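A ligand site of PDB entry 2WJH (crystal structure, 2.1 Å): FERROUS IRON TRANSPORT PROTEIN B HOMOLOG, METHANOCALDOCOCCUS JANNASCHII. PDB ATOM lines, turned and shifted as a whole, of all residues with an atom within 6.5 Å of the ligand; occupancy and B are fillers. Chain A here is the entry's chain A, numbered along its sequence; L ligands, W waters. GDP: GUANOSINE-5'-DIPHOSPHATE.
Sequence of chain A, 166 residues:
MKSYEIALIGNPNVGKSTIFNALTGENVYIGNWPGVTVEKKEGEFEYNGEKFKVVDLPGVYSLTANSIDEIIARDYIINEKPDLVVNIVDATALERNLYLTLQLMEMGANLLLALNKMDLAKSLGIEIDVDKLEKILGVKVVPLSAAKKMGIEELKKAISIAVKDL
OG of Ser 145 is in hydrogen-bond range of N of Asp 119 (3.2 Å).
The backbone NH (N) of Ser 145 lies within hydrogen-bond range of the backbone carbonyl oxygen (O) of Met 150.
The backbone carbonyl oxygen (O) of Asn 13 sits at hydrogen-bond distance from the side-chain amino group (NZ) of Lys 117, at 2.9 Å.
N of Lys 117 sits at hydrogen-bond distance from O of Leu 144, at 3.4 Å.
ND2 of Asn 116 lies within hydrogen-bond range of O of Val 14.
The side-chain amide oxygen (OD1) of Asn 116 is in hydrogen-bond range of the backbone NH (N) of Ala 146, 2.9 Å away.
The side-chain carboxylate of Asp 119 is in salt-bridge range of the side-chain amino group of Lys 148.
Leu 120 touches the ligand.
C of Ser 145 touches O6 of the ligand, 3.0 Å away.
Hydrophobic or aromatic side chains within 4 Å of the ligand: Val 14, Leu 120 and Ala 147.
Along chain A the residues within 4 Å of the ligand span positions 13 to 147.
The nearest printed residue that does not touch the ligand is Asn 11 (4.2 Å).
Water W3 bridges O2B of the ligand (2.5 Å) and O of Asn 11 (2.8 Å).
O6 of the ligand lies close to OD1 of Asn 116, at 3.3 Å.
The side-chain amino group (NZ) of Lys 117 lies within hydrogen-bond range of an oxygen (O4') of the ligand (3.2 Å).
The side-chain carboxylate of Asp 119 sits at hydrogen-bond distance from a nitrogen (N1) of the ligand (2.8 Å).
The backbone NH of Thr 18 is in hydrogen-bond range of an oxygen (O2A) of the ligand (2.9 Å).
N of Lys 16 is in hydrogen-bond range of O2B of the ligand (2.9 Å).
The backbone NH of Ala 146 lies within hydrogen-bond range of an oxygen (O6) of the ligand (2.8 Å).
The backbone NH of Ala 147 sits at hydrogen-bond distance from an oxygen (O6) of the ligand, at 3.1 Å.
An oxygen (O3B) of the ligand lies within hydrogen-bond range of the backbone NH of Asn 13, at 3.0 Å.
An oxygen (O2A) of the ligand sits at hydrogen-bond distance from the side-chain hydroxyl (OG1) of Thr 18 (2.9 Å).
O3A of the ligand sits at hydrogen-bond distance from N of Gly 15 (2.8 Å).
The backbone NH (N) of Ser 17 lies within hydrogen-bond range of an oxygen (O1B) of the ligand.
The backbone NH (N) of Val 14 sits at hydrogen-bond distance from an oxygen (O2B) of the ligand.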
ATOM      1  N   GLY A  10     -12.157  25.424 -12.840  1.00  0.00           N
ATOM      2  CA  GLY A  10     -13.372  25.846 -12.167  1.00  0.00           C
ATOM      3  C   GLY A  10     -14.041  24.655 -11.547  1.00  0.00           C
ATOM      4  O   GLY A  10     -13.545  23.551 -11.690  1.00  0.00           O
ATOM      5  N   ASN A  11     -15.157  24.881 -10.848  1.00  0.00           N
ATOM      6  CA  ASN A  11     -15.991  23.794 -10.355  1.00  0.00           C
ATOM      7  C   ASN A  11     -16.516  22.892 -11.486  1.00  0.00           C
ATOM      8  O   ASN A  11     -16.626  23.331 -12.643  1.00  0.00           O
ATOM      9  CB  ASN A  11     -17.189  24.354  -9.571  1.00  0.00           C
ATOM     10  CG  ASN A  11     -16.784  25.293  -8.422  1.00  0.00           C
ATOM     11  OD1 ASN A  11     -15.686  25.215  -7.871  1.00  0.00           O
ATOM     12  ND2 ASN A  11     -17.709  26.146  -8.023  1.00  0.00           N
ATOM     13  N   PRO A  12     -16.857  21.632 -11.160  1.00  0.00           N
ATOM     14  CA  PRO A  12     -17.503  20.794 -12.183  1.00  0.00           C
ATOM     15  C   PRO A  12     -18.795  21.437 -12.730  1.00  0.00           C
ATOM     16  O   PRO A  12     -19.510  22.097 -11.974  1.00  0.00           O
ATOM     17  CB  PRO A  12     -17.827  19.488 -11.415  1.00  0.00           C
ATOM     18  CG  PRO A  12     -16.771  19.431 -10.302  1.00  0.00           C
ATOM     19  CD  PRO A  12     -16.560  20.884  -9.919  1.00  0.00           C
ATOM     20  N   ASN A  13     -19.083  21.254 -14.025  1.00  0.00           N
ATOM     21  CA  ASN A  13     -20.348  21.729 -14.599  1.00  0.00           C
ATOM     22  C   ASN A  13     -20.511  23.257 -14.686  1.00  0.00           C
ATOM     23  O   ASN A  13     -21.619  23.766 -14.494  1.00  0.00           O
ATOM     24  CB  ASN A  13     -21.537  21.163 -13.801  1.00  0.00           C
ATOM     25  CG  ASN A  13     -21.351  19.691 -13.448  1.00  0.00           C
ATOM     26  OD1 ASN A  13     -21.402  19.297 -12.281  1.00  0.00           O
ATOM     27  ND2 ASN A  13     -21.128  18.874 -14.470  1.00  0.00           N
ATOM     28  N   VAL A  14     -19.432  23.975 -14.929  1.00  0.00           N
ATOM     29  CA  VAL A  14     -19.527  25.420 -15.112  1.00  0.00           C
ATOM     30  C   VAL A  14     -19.479  25.806 -16.601  1.00  0.00           C
ATOM     31  O   VAL A  14     -19.602  26.977 -16.933  1.00  0.00           O
ATOM     32  CB  VAL A  14     -18.413  26.175 -14.372  1.00  0.00           C
ATOM     33  CG1 VAL A  14     -18.498  25.921 -12.885  1.00  0.00           C
ATOM     34  CG2 VAL A  14     -17.046  25.759 -14.902  1.00  0.00           C
ATOM     35  N   GLY A  15     -19.319  24.820 -17.475  1.00  0.00           N
ATOM     36  CA  GLY A  15     -19.275  25.056 -18.907  1.00  0.00           C
ATOM     37  C   GLY A  15     -17.836  25.251 -19.335  1.00  0.00           C
ATOM     38  O   GLY A  15     -17.558  25.896 -20.325  1.00  0.00           O
ATOM     39  N   LYS A  16     -16.907  24.692 -18.556  1.00  0.00           N
ATOM     40  CA  LYS A  16     -15.484  24.803 -18.831  1.00  0.00           C
ATOM     41  C   LYS A  16     -15.132  24.196 -20.165  1.00  0.00           C
ATOM     42  O   LYS A  16     -14.334  24.751 -20.928  1.00  0.00           O
ATOM     43  CB  LYS A  16     -14.674  24.139 -17.701  1.00  0.00           C
ATOM     44  CG  LYS A  16     -13.186  24.391 -17.826  1.00  0.00           C
ATOM     45  CD  LYS A  16     -12.369  24.157 -16.555  1.00  0.00           C
ATOM     46  CE  LYS A  16     -12.506  22.768 -15.961  1.00  0.00           C
ATOM     47  NZ  LYS A  16     -12.040  21.635 -16.811  1.00  0.00           N
ATOM     48  N   SER A  17     -15.713  23.040 -20.452  1.00  0.00           N
ATOM     49  CA  SER A  17     -15.430  22.354 -21.707  1.00  0.00           C
ATOM     50  C   SER A  17     -15.865  23.194 -22.910  1.00  0.00           C
ATOM     51  O   SER A  17     -15.147  23.309 -23.915  1.00  0.00           O
ATOM     52  CB  SER A  17     -16.101  20.975 -21.736  1.00  0.00           C
ATOM     53  OG  SER A  17     -15.597  20.218 -22.813  1.00  0.00           O
ATOM     54  N   THR A  18     -17.037  23.799 -22.781  1.00  0.00           N
ATOM     55  CA  THR A  18     -17.596  24.664 -23.807  1.00  0.00           C
ATOM     56  C   THR A  18     -16.679  25.868 -24.055  1.00  0.00           C
ATOM     57  O   THR A  18     -16.407  26.241 -25.193  1.00  0.00           O
ATOM     58  CB  THR A  18     -18.970  25.161 -23.385  1.00  0.00           C
ATOM     59  OG1 THR A  18     -19.793  24.039 -23.026  1.00  0.00           O
ATOM     60  CG2 THR A  18     -19.646  25.963 -24.518  1.00  0.00           C
ATOM     61  N   ILE A  19     -16.201  26.468 -22.974  1.00  0.00           N
ATOM     62  CA  ILE A  19     -15.311  27.623 -23.086  1.00  0.00           C
ATOM     63  C   ILE A  19     -13.957  27.200 -23.637  1.00  0.00           C
ATOM     64  O   ILE A  19     -13.350  27.929 -24.448  1.00  0.00           O
ATOM     65  CB  ILE A  19     -15.148  28.351 -21.733  1.00  0.00           C
ATOM     66  CG1 ILE A  19     -16.325  29.284 -21.514  1.00  0.00           C
ATOM     67  CG2 ILE A  19     -13.898  29.203 -21.725  1.00  0.00           C
ATOM     68  CD1 ILE A  19     -16.615  29.576 -20.071  1.00  0.00           C
ATOM     69  N   GLY A  59     -11.898  19.947 -13.301  1.00  0.00           N
ATOM     70  CA  GLY A  59     -12.875  20.664 -12.491  1.00  0.00           C
ATOM     71  C   GLY A  59     -12.747  20.275 -11.015  1.00  0.00           C
ATOM     72  O   GLY A  59     -12.658  19.087 -10.707  1.00  0.00           O
ATOM     73  N   ASN A 116     -19.728  32.657 -16.183  1.00  0.00           N
ATOM     74  CA  ASN A 116     -20.467  31.943 -17.228  1.00  0.00           C
ATOM     75  C   ASN A 116     -21.929  31.707 -16.848  1.00  0.00           C
ATOM     76  O   ASN A 116     -22.335  31.920 -15.691  1.00  0.00           O
ATOM     77  CB  ASN A 116     -19.755  30.625 -17.593  1.00  0.00           C
ATOM     78  CG  ASN A 116     -20.151  30.068 -18.958  1.00  0.00           C
ATOM     79  OD1 ASN A 116     -20.448  30.816 -19.893  1.00  0.00           O
ATOM     80  ND2 ASN A 116     -20.159  28.750 -19.084  1.00  0.00           N
ATOM     81  N   LYS A 117     -22.729  31.302 -17.828  1.00  0.00           N
ATOM     82  CA  LYS A 117     -24.156  31.044 -17.626  1.00  0.00           C
ATOM     83  C   LYS A 117     -24.925  32.276 -17.118  1.00  0.00           C
ATOM     84  O   LYS A 117     -25.864  32.153 -16.340  1.00  0.00           O
ATOM     85  CB  LYS A 117     -24.342  29.856 -16.676  1.00  0.00           C
ATOM     86  CG  LYS A 117     -23.821  28.540 -17.260  1.00  0.00           C
ATOM     87  CD  LYS A 117     -24.100  27.355 -16.347  1.00  0.00           C
ATOM     88  CE  LYS A 117     -23.540  26.071 -16.960  1.00  0.00           C
ATOM     89  NZ  LYS A 117     -23.732  24.837 -16.110  1.00  0.00           N
ATOM     90  N   MET A 118     -24.512  33.462 -17.570  1.00  0.00           N
ATOM     91  CA  MET A 118     -25.242  34.691 -17.266  1.00  0.00           C
ATOM     92  C   MET A 118     -26.664  34.600 -17.797  1.00  0.00           C
ATOM     93  O   MET A 118     -27.600  35.014 -17.119  1.00  0.00           O
ATOM     94  CB  MET A 118     -24.531  35.908 -17.855  1.00  0.00           C
ATOM     95  CG  MET A 118     -23.162  36.181 -17.248  1.00  0.00           C
ATOM     96  SD  MET A 118     -23.269  36.933 -15.608  1.00  0.00           S
ATOM     97  CE  MET A 118     -23.648  38.626 -16.065  1.00  0.00           C
ATOM     98  N   ASP A 119     -26.831  34.038 -18.994  1.00  0.00           N
ATOM     99  CA  ASP A 119     -28.171  33.815 -19.546  1.00  0.00           C
ATOM    100  C   ASP A 119     -29.064  33.011 -18.582  1.00  0.00           C
ATOM    101  O   ASP A 119     -30.227  33.353 -18.366  1.00  0.00           O
ATOM    102  CB  ASP A 119     -28.093  33.108 -20.905  1.00  0.00           C
ATOM    103  CG  ASP A 119     -27.374  31.756 -20.829  1.00  0.00           C
ATOM    104  OD1 ASP A 119     -27.814  30.803 -21.519  1.00  0.00           O
ATOM    105  OD2 ASP A 119     -26.375  31.644 -20.071  1.00  0.00           O
ATOM    106  N   LEU A 120     -28.512  31.953 -17.997  1.00  0.00           N
ATOM    107  CA  LEU A 120     -29.260  31.090 -17.081  1.00  0.00           C
ATOM    108  C   LEU A 120     -29.639  31.837 -15.811  1.00  0.00           C
ATOM    109  O   LEU A 120     -30.766  31.714 -15.323  1.00  0.00           O
ATOM    110  CB  LEU A 120     -28.421  29.863 -16.701  1.00  0.00           C
ATOM    111  CG  LEU A 120     -29.105  28.505 -16.507  1.00  0.00           C
ATOM    112  CD1 LEU A 120     -28.281  27.666 -15.531  1.00  0.00           C
ATOM    113  CD2 LEU A 120     -30.538  28.646 -16.053  1.00  0.00           C
ATOM    114  N   ALA A 121     -28.700  32.613 -15.275  1.00  0.00           N
ATOM    115  CA  ALA A 121     -29.001  33.466 -14.143  1.00  0.00           C
ATOM    116  C   ALA A 121     -30.094  34.473 -14.515  1.00  0.00           C
ATOM    117  O   ALA A 121     -30.991  34.746 -13.732  1.00  0.00           O
ATOM    118  CB  ALA A 121     -27.756  34.188 -13.660  1.00  0.00           C
ATOM    119  N   LEU A 144     -20.199  36.241 -19.352  1.00  0.00           N
ATOM    120  CA  LEU A 144     -20.455  35.588 -20.626  1.00  0.00           C
ATOM    121  C   LEU A 144     -21.540  34.534 -20.562  1.00  0.00           C
ATOM    122  O   LEU A 144     -22.074  34.231 -19.496  1.00  0.00           O
ATOM    123  CB  LEU A 144     -19.184  35.007 -21.271  1.00  0.00           C
ATOM    124  CG  LEU A 144     -18.084  34.232 -20.563  1.00  0.00           C
ATOM    125  CD1 LEU A 144     -18.523  33.633 -19.256  1.00  0.00           C
ATOM    126  CD2 LEU A 144     -17.608  33.115 -21.473  1.00  0.00           C
ATOM    127  N   SER A 145     -21.895  34.022 -21.738  1.00  0.00           N
ATOM    128  CA  SER A 145     -22.787  32.889 -21.902  1.00  0.00           C
ATOM    129  C   SER A 145     -22.201  32.056 -23.017  1.00  0.00           C
ATOM    130  O   SER A 145     -22.625  32.145 -24.170  1.00  0.00           O
ATOM    131  CB  SER A 145     -24.189  33.362 -22.279  1.00  0.00           C
ATOM    132  OG  SER A 145     -24.678  34.272 -21.300  1.00  0.00           O
ATOM    133  N   ALA A 146     -21.199  31.245 -22.667  1.00  0.00           N
ATOM    134  CA  ALA A 146     -20.426  30.512 -23.674  1.00  0.00           C
ATOM    135  C   ALA A 146     -21.283  29.644 -24.572  1.00  0.00           C
ATOM    136  O   ALA A 146     -20.999  29.508 -25.746  1.00  0.00           O
ATOM    137  CB  ALA A 146     -19.356  29.681 -22.999  1.00  0.00           C
ATOM    138  N   ALA A 147     -22.338  29.061 -24.014  1.00  0.00           N
ATOM    139  CA  ALA A 147     -23.250  28.205 -24.784  1.00  0.00           C
ATOM    140  C   ALA A 147     -24.100  28.996 -25.778  1.00  0.00           C
ATOM    141  O   ALA A 147     -24.643  28.428 -26.730  1.00  0.00           O
ATOM    142  CB  ALA A 147     -24.136  27.391 -23.855  1.00  0.00           C
ATOM    143  N   LYS A 148     -24.220  30.308 -25.557  1.00  0.00           N
ATOM    144  CA  LYS A 148     -24.962  31.179 -26.468  1.00  0.00           C
ATOM    145  C   LYS A 148     -24.014  31.945 -27.390  1.00  0.00           C
ATOM    146  O   LYS A 148     -24.418  32.916 -28.029  1.00  0.00           O
ATOM    147  CB  LYS A 148     -25.854  32.149 -25.685  1.00  0.00           C
ATOM    148  CG  LYS A 148     -27.171  31.566 -25.208  1.00  0.00           C
ATOM    149  CD  LYS A 148     -26.975  30.201 -24.557  1.00  0.00           C
ATOM    150  CE  LYS A 148     -28.290  29.436 -24.408  1.00  0.00           C
ATOM    151  NZ  LYS A 148     -28.045  27.965 -24.235  1.00  0.00           N
ATOM    152  N   LYS A 149     -22.762  31.498 -27.462  1.00  0.00           N
ATOM    153  CA  LYS A 149     -21.747  32.164 -28.262  1.00  0.00           C
ATOM    154  C   LYS A 149     -21.650  33.637 -27.875  1.00  0.00           C
ATOM    155  O   LYS A 149     -21.425  34.504 -28.740  1.00  0.00           O
ATOM    156  CB  LYS A 149     -22.045  32.022 -29.750  1.00  0.00           C
ATOM    157  CG  LYS A 149     -21.508  30.746 -30.360  1.00  0.00           C
ATOM    158  CD  LYS A 149     -21.685  30.745 -31.868  1.00  0.00           C
ATOM    159  CE  LYS A 149     -20.516  30.040 -32.549  1.00  0.00           C
ATOM    160  NZ  LYS A 149     -20.240  28.700 -31.965  1.00  0.00           N
ATOM    161  N   MET A 150     -21.831  33.895 -26.583  1.00  0.00           N
ATOM    162  CA  MET A 150     -21.842  35.245 -26.044  1.00  0.00           C
ATOM    163  C   MET A 150     -20.601  35.513 -25.190  1.00  0.00           C
ATOM    164  O   MET A 150     -20.367  34.805 -24.193  1.00  0.00           O
ATOM    165  CB  MET A 150     -23.086  35.454 -25.208  1.00  0.00           C
ATOM    166  CG  MET A 150     -23.632  36.863 -25.243  1.00  0.00           C
ATOM    167  SD  MET A 150     -24.348  37.257 -26.844  1.00  0.00           S
ATOM    168  CE  MET A 150     -24.577  39.014 -26.647  1.00  0.00           C
HETATM  169  PB  GDP L   1     -17.917  21.480 -17.604  1.00  0.00           P
HETATM  170  O1B GDP L   1     -16.985  20.985 -18.674  1.00  0.00           O
HETATM  171  O2B GDP L   1     -17.184  22.449 -16.693  1.00  0.00           O
HETATM  172  O3B GDP L   1     -18.456  20.322 -16.798  1.00  0.00           O
HETATM  173  O3A GDP L   1     -19.148  22.191 -18.308  1.00  0.00           O
HETATM  174  PA  GDP L   1     -19.615  21.731 -19.787  1.00  0.00           P
HETATM  175  O1A GDP L   1     -19.591  20.233 -19.929  1.00  0.00           O
HETATM  176  O2A GDP L   1     -18.787  22.433 -20.853  1.00  0.00           O
HETATM  177  O5' GDP L   1     -21.108  22.295 -19.760  1.00  0.00           O
HETATM  178  C5' GDP L   1     -22.028  21.691 -18.853  1.00  0.00           C
HETATM  179  C4' GDP L   1     -23.426  22.125 -19.241  1.00  0.00           C
HETATM  180  O4' GDP L   1     -23.516  23.536 -19.067  1.00  0.00           O
HETATM  181  C3' GDP L   1     -23.636  21.822 -20.720  1.00  0.00           C
HETATM  182  O3' GDP L   1     -24.774  20.985 -20.899  1.00  0.00           O
HETATM  183  C2' GDP L   1     -23.853  23.177 -21.374  1.00  0.00           C
HETATM  184  O2' GDP L   1     -24.932  23.175 -22.317  1.00  0.00           O
HETATM  185  C1' GDP L   1     -24.139  24.108 -20.220  1.00  0.00           C
HETATM  186  N9  GDP L   1     -23.582  25.427 -20.542  1.00  0.00           N
HETATM  187  C8  GDP L   1     -22.324  25.728 -20.915  1.00  0.00           C
HETATM  188  N7  GDP L   1     -22.181  27.067 -21.134  1.00  0.00           N
HETATM  189  C5  GDP L   1     -23.388  27.629 -20.896  1.00  0.00           C
HETATM  190  C6  GDP L   1     -23.975  28.980 -20.924  1.00  0.00           C
HETATM  191  O6  GDP L   1     -23.285  29.954 -21.236  1.00  0.00           O
HETATM  192  N1  GDP L   1     -25.266  29.140 -20.611  1.00  0.00           N
HETATM  193  C2  GDP L   1     -26.056  28.106 -20.265  1.00  0.00           C
HETATM  194  N2  GDP L   1     -27.350  28.361 -19.958  1.00  0.00           N
HETATM  195  N3  GDP L   1     -25.593  26.831 -20.208  1.00  0.00           N
HETATM  196  C4  GDP L   1     -24.305  26.541 -20.505  1.00  0.00           C
HETATM  197  O   HOH W   1     -27.819  25.281 -18.557  1.00  0.00           O
HETATM  198  O   HOH W   2     -17.583  17.893 -16.003  1.00  0.00           O
HETATM  199  O   HOH W   3     -15.463  22.234 -14.945  1.00  0.00           O
HETATM  200  O   HOH W   4     -27.103  24.766 -22.611  1.00  0.00           O
